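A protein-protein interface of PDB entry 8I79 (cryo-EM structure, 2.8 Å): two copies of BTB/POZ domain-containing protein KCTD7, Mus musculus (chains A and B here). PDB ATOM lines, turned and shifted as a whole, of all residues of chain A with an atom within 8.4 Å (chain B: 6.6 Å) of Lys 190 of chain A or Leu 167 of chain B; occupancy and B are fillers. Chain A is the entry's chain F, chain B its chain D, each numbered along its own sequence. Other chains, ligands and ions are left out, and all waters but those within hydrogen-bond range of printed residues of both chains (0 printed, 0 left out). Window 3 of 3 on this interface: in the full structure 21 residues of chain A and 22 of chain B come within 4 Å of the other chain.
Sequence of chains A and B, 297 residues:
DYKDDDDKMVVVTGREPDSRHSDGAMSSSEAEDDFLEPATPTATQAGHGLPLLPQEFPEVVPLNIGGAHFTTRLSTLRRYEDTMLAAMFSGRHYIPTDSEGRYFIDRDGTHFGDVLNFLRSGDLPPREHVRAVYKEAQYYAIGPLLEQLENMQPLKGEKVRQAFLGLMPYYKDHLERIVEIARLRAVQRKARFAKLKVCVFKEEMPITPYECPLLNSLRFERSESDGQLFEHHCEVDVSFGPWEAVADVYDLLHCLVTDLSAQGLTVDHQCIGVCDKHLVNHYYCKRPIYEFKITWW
N of Ala 191 of chain A is in hydrogen-bond range of O of Ala 186 of chain A, at 3.0 Å. NE1 of Trp 297 of chain A is in hydrogen-bond range of O of Ala 191 of chain A (3.3 Å). The backbone NH of Trp 296 of chain A sits at hydrogen-bond distance from the backbone carbonyl oxygen of Arg 192 of chain A. The guanidinium group of Arg 192 of chain A lies within hydrogen-bond range of the backbone carbonyl oxygen of Trp 297 of chain A (2.5 Å). The indole nitrogen of Trp 243 of chain B is in hydrogen-bond range of the backbone carbonyl oxygen of Ala 247 of chain B, 3.1 Å away.
Among the printed residues, merely in contact across the chains: Arg 189 of chain A with Val 246 of chain B (3.2 Å), Ala 191 of chain A with Val 246 of chain B (3.5 Å), Trp 297 of chain A with Phe 164 of chain B (3.5 Å), Lys 190 of chain A with Ala 247 of chain B (3.5 Å), Lys 190 of chain A with Val 246 of chain B (3.5 Å), Lys 190 of chain A with Ala 245 of chain B (3.6 Å), Trp 296 of chain A with Val 160 of chain B (3.7 Å), Lys 190 of chain A with Leu 167 of chain B (3.7 Å), Ala 186 of chain A with Val 160 of chain B (3.7 Å), Lys 190 of chain A with Ala 163 of chain B (3.7 Å), Trp 297 of chain A with Val 160 of chain B (3.9 Å), Arg 183 of chain A with Val 160 of chain B (3.9 Å) and Ala 191 of chain A with Val 160 of chain B (3.9 Å).
Of the printed residues of chain B, Arg 183 of chain A touches Val 160 (3.9 Å). Leu 184 of chain A touches none of the printed residues of chain B. Lys 190 of chain A touches just these residues of chain B: Ala 163, Leu 167, Ala 245, Val 246 and Ala 247. Arg 192 of chain A touches none of the printed residues of chain B. Printed residues of chain B within 4 Å of Trp 296 of chain A: Val 160. Of the printed residues of chain B, Trp 297 of chain A touches Val 160 and Phe 164. Of the printed residues of chain A, Ala 163 of chain B touches Lys 190. No residue of chain A comes within 4 Å of Gly 166 of chain B. Leu 167 of chain B touches just one residue of chain A: Lys 190 (3.7 Å). Of the printed residues of chain A, Val 246 of chain B touches Arg 189, Lys 190 and Ala 191. The nearest residue of chain A that does not touch Leu 167 of chain B is Arg 189 of chain A (7.2 Å). The nearest printed residue of chain B that does not touch Arg 183 of chain A is Ala 163 of chain B (7.4 Å).
Of the 13 printed residues of chain A, 7 touch a printed residue of chain B. Printed residues of chain A that touch a printed residue of chain B: Arg 183, Ala 186, Arg 189, Lys 190, Ala 191, Trp 296 and Trp 297. Among the printed residues, 13 pairs touch across the chains. Among the printed residues, no Asp or Glu carboxylate lies within 4 Å of a Lys or Arg side-chain nitrogen of the other chain.
No position is printed for both chains. Of the 13 pairs that touch across the chains among the printed residues, none has its exchanged pair printed and touching as well.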
ATOM      1  N   ARG A 183     -21.080  -3.582 -12.450  1.00  0.00           N
ATOM      2  CA  ARG A 183     -22.029  -2.813 -13.249  1.00  0.00           C
ATOM      3  C   ARG A 183     -22.529  -1.590 -12.492  1.00  0.00           C
ATOM      4  O   ARG A 183     -22.622  -0.496 -13.060  1.00  0.00           O
ATOM      5  CB  ARG A 183     -23.199  -3.698 -13.668  1.00  0.00           C
ATOM      6  CG  ARG A 183     -23.985  -3.160 -14.843  1.00  0.00           C
ATOM      7  CD  ARG A 183     -25.318  -3.866 -14.976  1.00  0.00           C
ATOM      8  NE  ARG A 183     -26.074  -3.826 -13.731  1.00  0.00           N
ATOM      9  CZ  ARG A 183     -26.924  -2.863 -13.402  1.00  0.00           C
ATOM     10  NH1 ARG A 183     -27.145  -1.832 -14.201  1.00  0.00           N
ATOM     11  NH2 ARG A 183     -27.569  -2.936 -12.241  1.00  0.00           N
ATOM     12  N   LEU A 184     -22.858  -1.755 -11.210  1.00  0.00           N
ATOM     13  CA  LEU A 184     -23.338  -0.626 -10.422  1.00  0.00           C
ATOM     14  C   LEU A 184     -22.271   0.447 -10.289  1.00  0.00           C
ATOM     15  O   LEU A 184     -22.565   1.640 -10.414  1.00  0.00           O
ATOM     16  CB  LEU A 184     -23.790  -1.097  -9.041  1.00  0.00           C
ATOM     17  CG  LEU A 184     -25.067  -1.930  -8.982  1.00  0.00           C
ATOM     18  CD1 LEU A 184     -25.474  -2.167  -7.539  1.00  0.00           C
ATOM     19  CD2 LEU A 184     -26.179  -1.242  -9.750  1.00  0.00           C
ATOM     20  N   ARG A 185     -21.024   0.048 -10.035  1.00  0.00           N
ATOM     21  CA  ARG A 185     -19.956   1.032  -9.906  1.00  0.00           C
ATOM     22  C   ARG A 185     -19.735   1.775 -11.217  1.00  0.00           C
ATOM     23  O   ARG A 185     -19.589   3.002 -11.231  1.00  0.00           O
ATOM     24  CB  ARG A 185     -18.668   0.354  -9.445  1.00  0.00           C
ATOM     25  CG  ARG A 185     -18.613   0.109  -7.955  1.00  0.00           C
ATOM     26  CD  ARG A 185     -17.311  -0.550  -7.554  1.00  0.00           C
ATOM     27  NE  ARG A 185     -17.318  -0.939  -6.151  1.00  0.00           N
ATOM     28  CZ  ARG A 185     -16.290  -1.491  -5.523  1.00  0.00           C
ATOM     29  NH1 ARG A 185     -15.150  -1.732  -6.147  1.00  0.00           N
ATOM     30  NH2 ARG A 185     -16.408  -1.805  -4.237  1.00  0.00           N
ATOM     31  N   ALA A 186     -19.723   1.046 -12.335  1.00  0.00           N
ATOM     32  CA  ALA A 186     -19.507   1.689 -13.625  1.00  0.00           C
ATOM     33  C   ALA A 186     -20.644   2.642 -13.972  1.00  0.00           C
ATOM     34  O   ALA A 186     -20.405   3.732 -14.501  1.00  0.00           O
ATOM     35  CB  ALA A 186     -19.345   0.636 -14.716  1.00  0.00           C
ATOM     36  N   VAL A 187     -21.889   2.248 -13.695  1.00  0.00           N
ATOM     37  CA  VAL A 187     -23.023   3.104 -14.036  1.00  0.00           C
ATOM     38  C   VAL A 187     -23.064   4.332 -13.134  1.00  0.00           C
ATOM     39  O   VAL A 187     -23.261   5.457 -13.608  1.00  0.00           O
ATOM     40  CB  VAL A 187     -24.335   2.305 -13.967  1.00  0.00           C
ATOM     41  CG1 VAL A 187     -25.525   3.240 -14.032  1.00  0.00           C
ATOM     42  CG2 VAL A 187     -24.395   1.301 -15.098  1.00  0.00           C
ATOM     43  N   GLN A 188     -22.881   4.141 -11.826  1.00  0.00           N
ATOM     44  CA  GLN A 188     -22.940   5.267 -10.901  1.00  0.00           C
ATOM     45  C   GLN A 188     -21.800   6.245 -11.141  1.00  0.00           C
ATOM     46  O   GLN A 188     -22.006   7.464 -11.127  1.00  0.00           O
ATOM     47  CB  GLN A 188     -22.913   4.762  -9.460  1.00  0.00           C
ATOM     48  CG  GLN A 188     -24.213   4.129  -9.004  1.00  0.00           C
ATOM     49  CD  GLN A 188     -24.056   3.351  -7.716  1.00  0.00           C
ATOM     50  OE1 GLN A 188     -22.969   3.292  -7.142  1.00  0.00           O
ATOM     51  NE2 GLN A 188     -25.145   2.749  -7.252  1.00  0.00           N
ATOM     52  N   ARG A 189     -20.589   5.735 -11.360  1.00  0.00           N
ATOM     53  CA  ARG A 189     -19.451   6.605 -11.609  1.00  0.00           C
ATOM     54  C   ARG A 189     -19.362   7.067 -13.055  1.00  0.00           C
ATOM     55  O   ARG A 189     -18.617   8.012 -13.335  1.00  0.00           O
ATOM     56  CB  ARG A 189     -18.153   5.896 -11.225  1.00  0.00           C
ATOM     57  CG  ARG A 189     -17.968   5.685  -9.738  1.00  0.00           C
ATOM     58  CD  ARG A 189     -16.506   5.461  -9.425  1.00  0.00           C
ATOM     59  NE  ARG A 189     -15.873   4.614 -10.429  1.00  0.00           N
ATOM     60  CZ  ARG A 189     -14.573   4.600 -10.685  1.00  0.00           C
ATOM     61  NH1 ARG A 189     -13.733   5.392 -10.040  1.00  0.00           N
ATOM     62  NH2 ARG A 189     -14.105   3.773 -11.616  1.00  0.00           N
ATOM     63  N   LYS A 190     -20.102   6.436 -13.967  1.00  0.00           N
ATOM     64  CA  LYS A 190     -20.034   6.723 -15.399  1.00  0.00           C
ATOM     65  C   LYS A 190     -18.615   6.510 -15.927  1.00  0.00           C
ATOM     66  O   LYS A 190     -17.948   7.428 -16.405  1.00  0.00           O
ATOM     67  CB  LYS A 190     -20.544   8.135 -15.698  1.00  0.00           C
ATOM     68  CG  LYS A 190     -22.007   8.331 -15.351  1.00  0.00           C
ATOM     69  CD  LYS A 190     -22.454   9.753 -15.610  1.00  0.00           C
ATOM     70  CE  LYS A 190     -23.930   9.921 -15.309  1.00  0.00           C
ATOM     71  NZ  LYS A 190     -24.210   9.753 -13.859  1.00  0.00           N
ATOM     72  N   ALA A 191     -18.163   5.261 -15.827  1.00  0.00           N
ATOM     73  CA  ALA A 191     -16.837   4.861 -16.269  1.00  0.00           C
ATOM     74  C   ALA A 191     -16.966   3.726 -17.271  1.00  0.00           C
ATOM     75  O   ALA A 191     -18.057   3.203 -17.509  1.00  0.00           O
ATOM     76  CB  ALA A 191     -15.955   4.414 -15.099  1.00  0.00           C
ATOM     77  N   ARG A 192     -15.833   3.357 -17.872  1.00  0.00           N
ATOM     78  CA  ARG A 192     -15.827   2.194 -18.752  1.00  0.00           C
ATOM     79  C   ARG A 192     -15.448   0.930 -17.992  1.00  0.00           C
ATOM     80  O   ARG A 192     -15.936  -0.160 -18.309  1.00  0.00           O
ATOM     81  CB  ARG A 192     -14.877   2.417 -19.927  1.00  0.00           C
ATOM     82  CG  ARG A 192     -13.449   2.687 -19.525  1.00  0.00           C
ATOM     83  CD  ARG A 192     -12.579   2.981 -20.728  1.00  0.00           C
ATOM     84  NE  ARG A 192     -12.812   2.063 -21.834  1.00  0.00           N
ATOM     85  CZ  ARG A 192     -12.065   2.014 -22.927  1.00  0.00           C
ATOM     86  NH1 ARG A 192     -11.042   2.834 -23.102  1.00  0.00           N
ATOM     87  NH2 ARG A 192     -12.349   1.118 -23.868  1.00  0.00           N
ATOM     88  N   PHE A 193     -14.584   1.051 -16.988  1.00  0.00           N
ATOM     89  CA  PHE A 193     -14.118  -0.092 -16.219  1.00  0.00           C
ATOM     90  C   PHE A 193     -14.431   0.109 -14.745  1.00  0.00           C
ATOM     91  O   PHE A 193     -14.352   1.228 -14.229  1.00  0.00           O
ATOM     92  CB  PHE A 193     -12.612  -0.322 -16.407  1.00  0.00           C
ATOM     93  CG  PHE A 193     -11.754   0.801 -15.901  1.00  0.00           C
ATOM     94  CD1 PHE A 193     -11.410   1.853 -16.730  1.00  0.00           C
ATOM     95  CD2 PHE A 193     -11.274   0.797 -14.603  1.00  0.00           C
ATOM     96  CE1 PHE A 193     -10.617   2.884 -16.271  1.00  0.00           C
ATOM     97  CE2 PHE A 193     -10.483   1.825 -14.137  1.00  0.00           C
ATOM     98  CZ  PHE A 193     -10.153   2.868 -14.971  1.00  0.00           C
ATOM     99  N   TRP A 296     -16.249  -2.529 -19.494  1.00  0.00           N
ATOM    100  CA  TRP A 296     -17.559  -2.616 -20.128  1.00  0.00           C
ATOM    101  C   TRP A 296     -17.509  -2.155 -21.577  1.00  0.00           C
ATOM    102  O   TRP A 296     -18.216  -2.699 -22.433  1.00  0.00           O
ATOM    103  CB  TRP A 296     -18.570  -1.796 -19.334  1.00  0.00           C
ATOM    104  CG  TRP A 296     -18.748  -2.302 -17.950  1.00  0.00           C
ATOM    105  CD1 TRP A 296     -18.267  -1.746 -16.808  1.00  0.00           C
ATOM    106  CD2 TRP A 296     -19.450  -3.482 -17.557  1.00  0.00           C
ATOM    107  NE1 TRP A 296     -18.629  -2.503 -15.724  1.00  0.00           N
ATOM    108  CE2 TRP A 296     -19.358  -3.577 -16.159  1.00  0.00           C
ATOM    109  CE3 TRP A 296     -20.151  -4.469 -18.255  1.00  0.00           C
ATOM    110  CZ2 TRP A 296     -19.939  -4.616 -15.444  1.00  0.00           C
ATOM    111  CZ3 TRP A 296     -20.725  -5.496 -17.544  1.00  0.00           C
ATOM    112  CH2 TRP A 296     -20.619  -5.563 -16.154  1.00  0.00           C
ATOM    113  N   TRP A 297     -16.685  -1.156 -21.871  1.00  0.00           N
ATOM    114  CA  TRP A 297     -16.574  -0.629 -23.223  1.00  0.00           C
ATOM    115  C   TRP A 297     -15.264   0.122 -23.404  1.00  0.00           C
ATOM    116  O   TRP A 297     -14.197  -0.485 -23.485  1.00  0.00           O
ATOM    117  CB  TRP A 297     -17.754   0.287 -23.541  1.00  0.00           C
ATOM    118  CG  TRP A 297     -17.988   1.349 -22.515  1.00  0.00           C
ATOM    119  CD1 TRP A 297     -18.748   1.248 -21.389  1.00  0.00           C
ATOM    120  CD2 TRP A 297     -17.456   2.679 -22.520  1.00  0.00           C
ATOM    121  NE1 TRP A 297     -18.727   2.430 -20.693  1.00  0.00           N
ATOM    122  CE2 TRP A 297     -17.940   3.325 -21.367  1.00  0.00           C
ATOM    123  CE3 TRP A 297     -16.619   3.386 -23.387  1.00  0.00           C
ATOM    124  CZ2 TRP A 297     -17.613   4.642 -21.059  1.00  0.00           C
ATOM    125  CZ3 TRP A 297     -16.297   4.691 -23.078  1.00  0.00           C
ATOM    126  CH2 TRP A 297     -16.793   5.306 -21.926  1.00  0.00           C
ATOM    127  N   VAL B 160     -24.207   0.354 -20.023  1.00  0.00           N
ATOM    128  CA  VAL B 160     -23.165   0.996 -19.226  1.00  0.00           C
ATOM    129  C   VAL B 160     -22.552   2.172 -19.980  1.00  0.00           C
ATOM    130  O   VAL B 160     -22.269   3.220 -19.388  1.00  0.00           O
ATOM    131  CB  VAL B 160     -22.103  -0.029 -18.800  1.00  0.00           C
ATOM    132  CG1 VAL B 160     -21.001   0.653 -18.021  1.00  0.00           C
ATOM    133  CG2 VAL B 160     -22.737  -1.106 -17.950  1.00  0.00           C
ATOM    134  N   GLN B 162     -24.040   3.915 -22.472  1.00  0.00           N
ATOM    135  CA  GLN B 162     -25.063   4.948 -22.586  1.00  0.00           C
ATOM    136  C   GLN B 162     -25.244   5.707 -21.285  1.00  0.00           C
ATOM    137  O   GLN B 162     -25.766   6.826 -21.300  1.00  0.00           O
ATOM    138  CB  GLN B 162     -26.401   4.344 -23.020  1.00  0.00           C
ATOM    139  CG  GLN B 162     -26.430   3.776 -24.435  1.00  0.00           C
ATOM    140  CD  GLN B 162     -25.814   4.698 -25.472  1.00  0.00           C
ATOM    141  OE1 GLN B 162     -25.949   5.920 -25.399  1.00  0.00           O
ATOM    142  NE2 GLN B 162     -25.134   4.111 -26.450  1.00  0.00           N
ATOM    143  N   ALA B 163     -24.843   5.116 -20.159  1.00  0.00           N
ATOM    144  CA  ALA B 163     -24.781   5.887 -18.923  1.00  0.00           C
ATOM    145  C   ALA B 163     -23.813   7.056 -19.062  1.00  0.00           C
ATOM    146  O   ALA B 163     -24.101   8.168 -18.606  1.00  0.00           O
ATOM    147  CB  ALA B 163     -24.376   4.989 -17.757  1.00  0.00           C
ATOM    148  N   PHE B 164     -22.656   6.821 -19.686  1.00  0.00           N
ATOM    149  CA  PHE B 164     -21.713   7.904 -19.944  1.00  0.00           C
ATOM    150  C   PHE B 164     -22.231   8.848 -21.021  1.00  0.00           C
ATOM    151  O   PHE B 164     -22.216  10.072 -20.848  1.00  0.00           O
ATOM    152  CB  PHE B 164     -20.354   7.333 -20.346  1.00  0.00           C
ATOM    153  CG  PHE B 164     -19.411   8.354 -20.910  1.00  0.00           C
ATOM    154  CD1 PHE B 164     -19.127   9.516 -20.217  1.00  0.00           C
ATOM    155  CD2 PHE B 164     -18.813   8.156 -22.141  1.00  0.00           C
ATOM    156  CE1 PHE B 164     -18.261  10.456 -20.740  1.00  0.00           C
ATOM    157  CE2 PHE B 164     -17.947   9.093 -22.667  1.00  0.00           C
ATOM    158  CZ  PHE B 164     -17.672  10.242 -21.967  1.00  0.00           C
ATOM    159  N   LEU B 165     -22.697   8.297 -22.141  1.00  0.00           N
ATOM    160  CA  LEU B 165     -23.124   9.121 -23.266  1.00  0.00           C
ATOM    161  C   LEU B 165     -24.492   9.749 -23.059  1.00  0.00           C
ATOM    162  O   LEU B 165     -24.917  10.551 -23.895  1.00  0.00           O
ATOM    163  CB  LEU B 165     -23.133   8.299 -24.555  1.00  0.00           C
ATOM    164  CG  LEU B 165     -21.841   7.554 -24.883  1.00  0.00           C
ATOM    165  CD1 LEU B 165     -22.095   6.493 -25.935  1.00  0.00           C
ATOM    166  CD2 LEU B 165     -20.778   8.528 -25.343  1.00  0.00           C
ATOM    167  N   GLY B 166     -25.196   9.399 -21.982  1.00  0.00           N
ATOM    168  CA  GLY B 166     -26.454  10.062 -21.687  1.00  0.00           C
ATOM    169  C   GLY B 166     -26.268  11.501 -21.255  1.00  0.00           C
ATOM    170  O   GLY B 166     -27.204  12.302 -21.334  1.00  0.00           O
ATOM    171  N   LEU B 167     -25.066  11.849 -20.791  1.00  0.00           N
ATOM    172  CA  LEU B 167     -24.762  13.236 -20.465  1.00  0.00           C
ATOM    173  C   LEU B 167     -24.748  14.117 -21.703  1.00  0.00           C
ATOM    174  O   LEU B 167     -24.787  15.346 -21.580  1.00  0.00           O
ATOM    175  CB  LEU B 167     -23.410  13.324 -19.759  1.00  0.00           C
ATOM    176  CG  LEU B 167     -23.209  12.432 -18.537  1.00  0.00           C
ATOM    177  CD1 LEU B 167     -21.737  12.121 -18.355  1.00  0.00           C
ATOM    178  CD2 LEU B 167     -23.775  13.092 -17.293  1.00  0.00           C
ATOM    179  N   MET B 168     -24.682  13.519 -22.883  1.00  0.00           N
ATOM    180  CA  MET B 168     -24.569  14.249 -24.143  1.00  0.00           C
ATOM    181  C   MET B 168     -25.669  13.806 -25.091  1.00  0.00           C
ATOM    182  O   MET B 168     -25.470  12.846 -25.859  1.00  0.00           O
ATOM    183  CB  MET B 168     -23.194  14.005 -24.758  1.00  0.00           C
ATOM    184  CG  MET B 168     -22.065  14.594 -23.938  1.00  0.00           C
ATOM    185  SD  MET B 168     -20.456  14.353 -24.690  1.00  0.00           S
ATOM    186  CE  MET B 168     -20.232  12.612 -24.359  1.00  0.00           C
ATOM    187  N   PRO B 169     -26.839  14.451 -25.082  1.00  0.00           N
ATOM    188  CA  PRO B 169     -27.915  14.042 -25.998  1.00  0.00           C
ATOM    189  C   PRO B 169     -27.618  14.338 -27.457  1.00  0.00           C
ATOM    190  O   PRO B 169     -28.359  13.863 -28.328  1.00  0.00           O
ATOM    191  CB  PRO B 169     -29.127  14.848 -25.508  1.00  0.00           C
ATOM    192  CG  PRO B 169     -28.716  15.457 -24.195  1.00  0.00           C
ATOM    193  CD  PRO B 169     -27.235  15.585 -24.235  1.00  0.00           C
ATOM    194  N   TYR B 170     -26.573  15.104 -27.750  1.00  0.00           N
ATOM    195  CA  TYR B 170     -26.207  15.457 -29.112  1.00  0.00           C
ATOM    196  C   TYR B 170     -25.164  14.520 -29.706  1.00  0.00           C
ATOM    197  O   TYR B 170     -24.648  14.798 -30.791  1.00  0.00           O
ATOM    198  CB  TYR B 170     -25.689  16.894 -29.158  1.00  0.00           C
ATOM    199  CG  TYR B 170     -24.715  17.236 -28.052  1.00  0.00           C
ATOM    200  CD1 TYR B 170     -23.400  16.800 -28.098  1.00  0.00           C
ATOM    201  CD2 TYR B 170     -25.109  18.006 -26.969  1.00  0.00           C
ATOM    202  CE1 TYR B 170     -22.508  17.113 -27.100  1.00  0.00           C
ATOM    203  CE2 TYR B 170     -24.221  18.323 -25.961  1.00  0.00           C
ATOM    204  CZ  TYR B 170     -22.922  17.874 -26.033  1.00  0.00           C
ATOM    205  OH  TYR B 170     -22.032  18.187 -25.035  1.00  0.00           O
ATOM    206  N   PRO B 242     -18.797  19.876 -22.684  1.00  0.00           N
ATOM    207  CA  PRO B 242     -18.359  19.382 -21.376  1.00  0.00           C
ATOM    208  C   PRO B 242     -19.315  18.341 -20.818  1.00  0.00           C
ATOM    209  O   PRO B 242     -20.504  18.319 -21.144  1.00  0.00           O
ATOM    210  CB  PRO B 242     -18.340  20.646 -20.514  1.00  0.00           C
ATOM    211  CG  PRO B 242     -19.372  21.518 -21.125  1.00  0.00           C
ATOM    212  CD  PRO B 242     -19.363  21.233 -22.604  1.00  0.00           C
ATOM    213  N   TRP B 243     -18.777  17.471 -19.968  1.00  0.00           N
ATOM    214  CA  TRP B 243     -19.561  16.462 -19.278  1.00  0.00           C
ATOM    215  C   TRP B 243     -18.968  16.240 -17.895  1.00  0.00           C
ATOM    216  O   TRP B 243     -17.781  16.487 -17.668  1.00  0.00           O
ATOM    217  CB  TRP B 243     -19.605  15.144 -20.064  1.00  0.00           C
ATOM    218  CG  TRP B 243     -18.286  14.447 -20.162  1.00  0.00           C
ATOM    219  CD1 TRP B 243     -17.713  13.638 -19.226  1.00  0.00           C
ATOM    220  CD2 TRP B 243     -17.368  14.500 -21.260  1.00  0.00           C
ATOM    221  NE1 TRP B 243     -16.499  13.182 -19.673  1.00  0.00           N
ATOM    222  CE2 TRP B 243     -16.264  13.697 -20.919  1.00  0.00           C
ATOM    223  CE3 TRP B 243     -17.374  15.148 -22.496  1.00  0.00           C
ATOM    224  CZ2 TRP B 243     -15.177  13.527 -21.771  1.00  0.00           C
ATOM    225  CZ3 TRP B 243     -16.295  14.977 -23.338  1.00  0.00           C
ATOM    226  CH2 TRP B 243     -15.213  14.173 -22.973  1.00  0.00           C
ATOM    227  N   GLU B 244     -19.804  15.773 -16.973  1.00  0.00           N
ATOM    228  CA  GLU B 244     -19.383  15.487 -15.606  1.00  0.00           C
ATOM    229  C   GLU B 244     -19.436  13.981 -15.394  1.00  0.00           C
ATOM    230  O   GLU B 244     -20.514  13.414 -15.189  1.00  0.00           O
ATOM    231  CB  GLU B 244     -20.259  16.218 -14.591  1.00  0.00           C
ATOM    232  CG  GLU B 244     -19.843  15.993 -13.147  1.00  0.00           C
ATOM    233  CD  GLU B 244     -18.472  16.565 -12.833  1.00  0.00           C
ATOM    234  OE1 GLU B 244     -18.049  17.521 -13.516  1.00  0.00           O
ATOM    235  OE2 GLU B 244     -17.814  16.052 -11.904  1.00  0.00           O
ATOM    236  N   ALA B 245     -18.272  13.342 -15.444  1.00  0.00           N
ATOM    237  CA  ALA B 245     -18.142  11.906 -15.250  1.00  0.00           C
ATOM    238  C   ALA B 245     -16.677  11.624 -14.958  1.00  0.00           C
ATOM    239  O   ALA B 245     -15.851  12.539 -14.900  1.00  0.00           O
ATOM    240  CB  ALA B 245     -18.624  11.119 -16.470  1.00  0.00           C
ATOM    241  N   VAL B 246     -16.359  10.340 -14.763  1.00  0.00           N
ATOM    242  CA  VAL B 246     -14.973   9.944 -14.540  1.00  0.00           C
ATOM    243  C   VAL B 246     -14.316   9.411 -15.804  1.00  0.00           C
ATOM    244  O   VAL B 246     -13.126   9.067 -15.775  1.00  0.00           O
ATOM    245  CB  VAL B 246     -14.863   8.897 -13.414  1.00  0.00           C
ATOM    246  CG1 VAL B 246     -15.471   9.435 -12.129  1.00  0.00           C
ATOM    247  CG2 VAL B 246     -15.530   7.618 -13.826  1.00  0.00           C
ATOM    248  N   ALA B 247     -15.047   9.329 -16.911  1.00  0.00           N
ATOM    249  CA  ALA B 247     -14.445   8.972 -18.182  1.00  0.00           C
ATOM    250  C   ALA B 247     -13.703  10.171 -18.765  1.00  0.00           C
ATOM    251  O   ALA B 247     -14.218  11.289 -18.821  1.00  0.00           O
ATOM    252  CB  ALA B 247     -15.504   8.478 -19.164  1.00  0.00           C
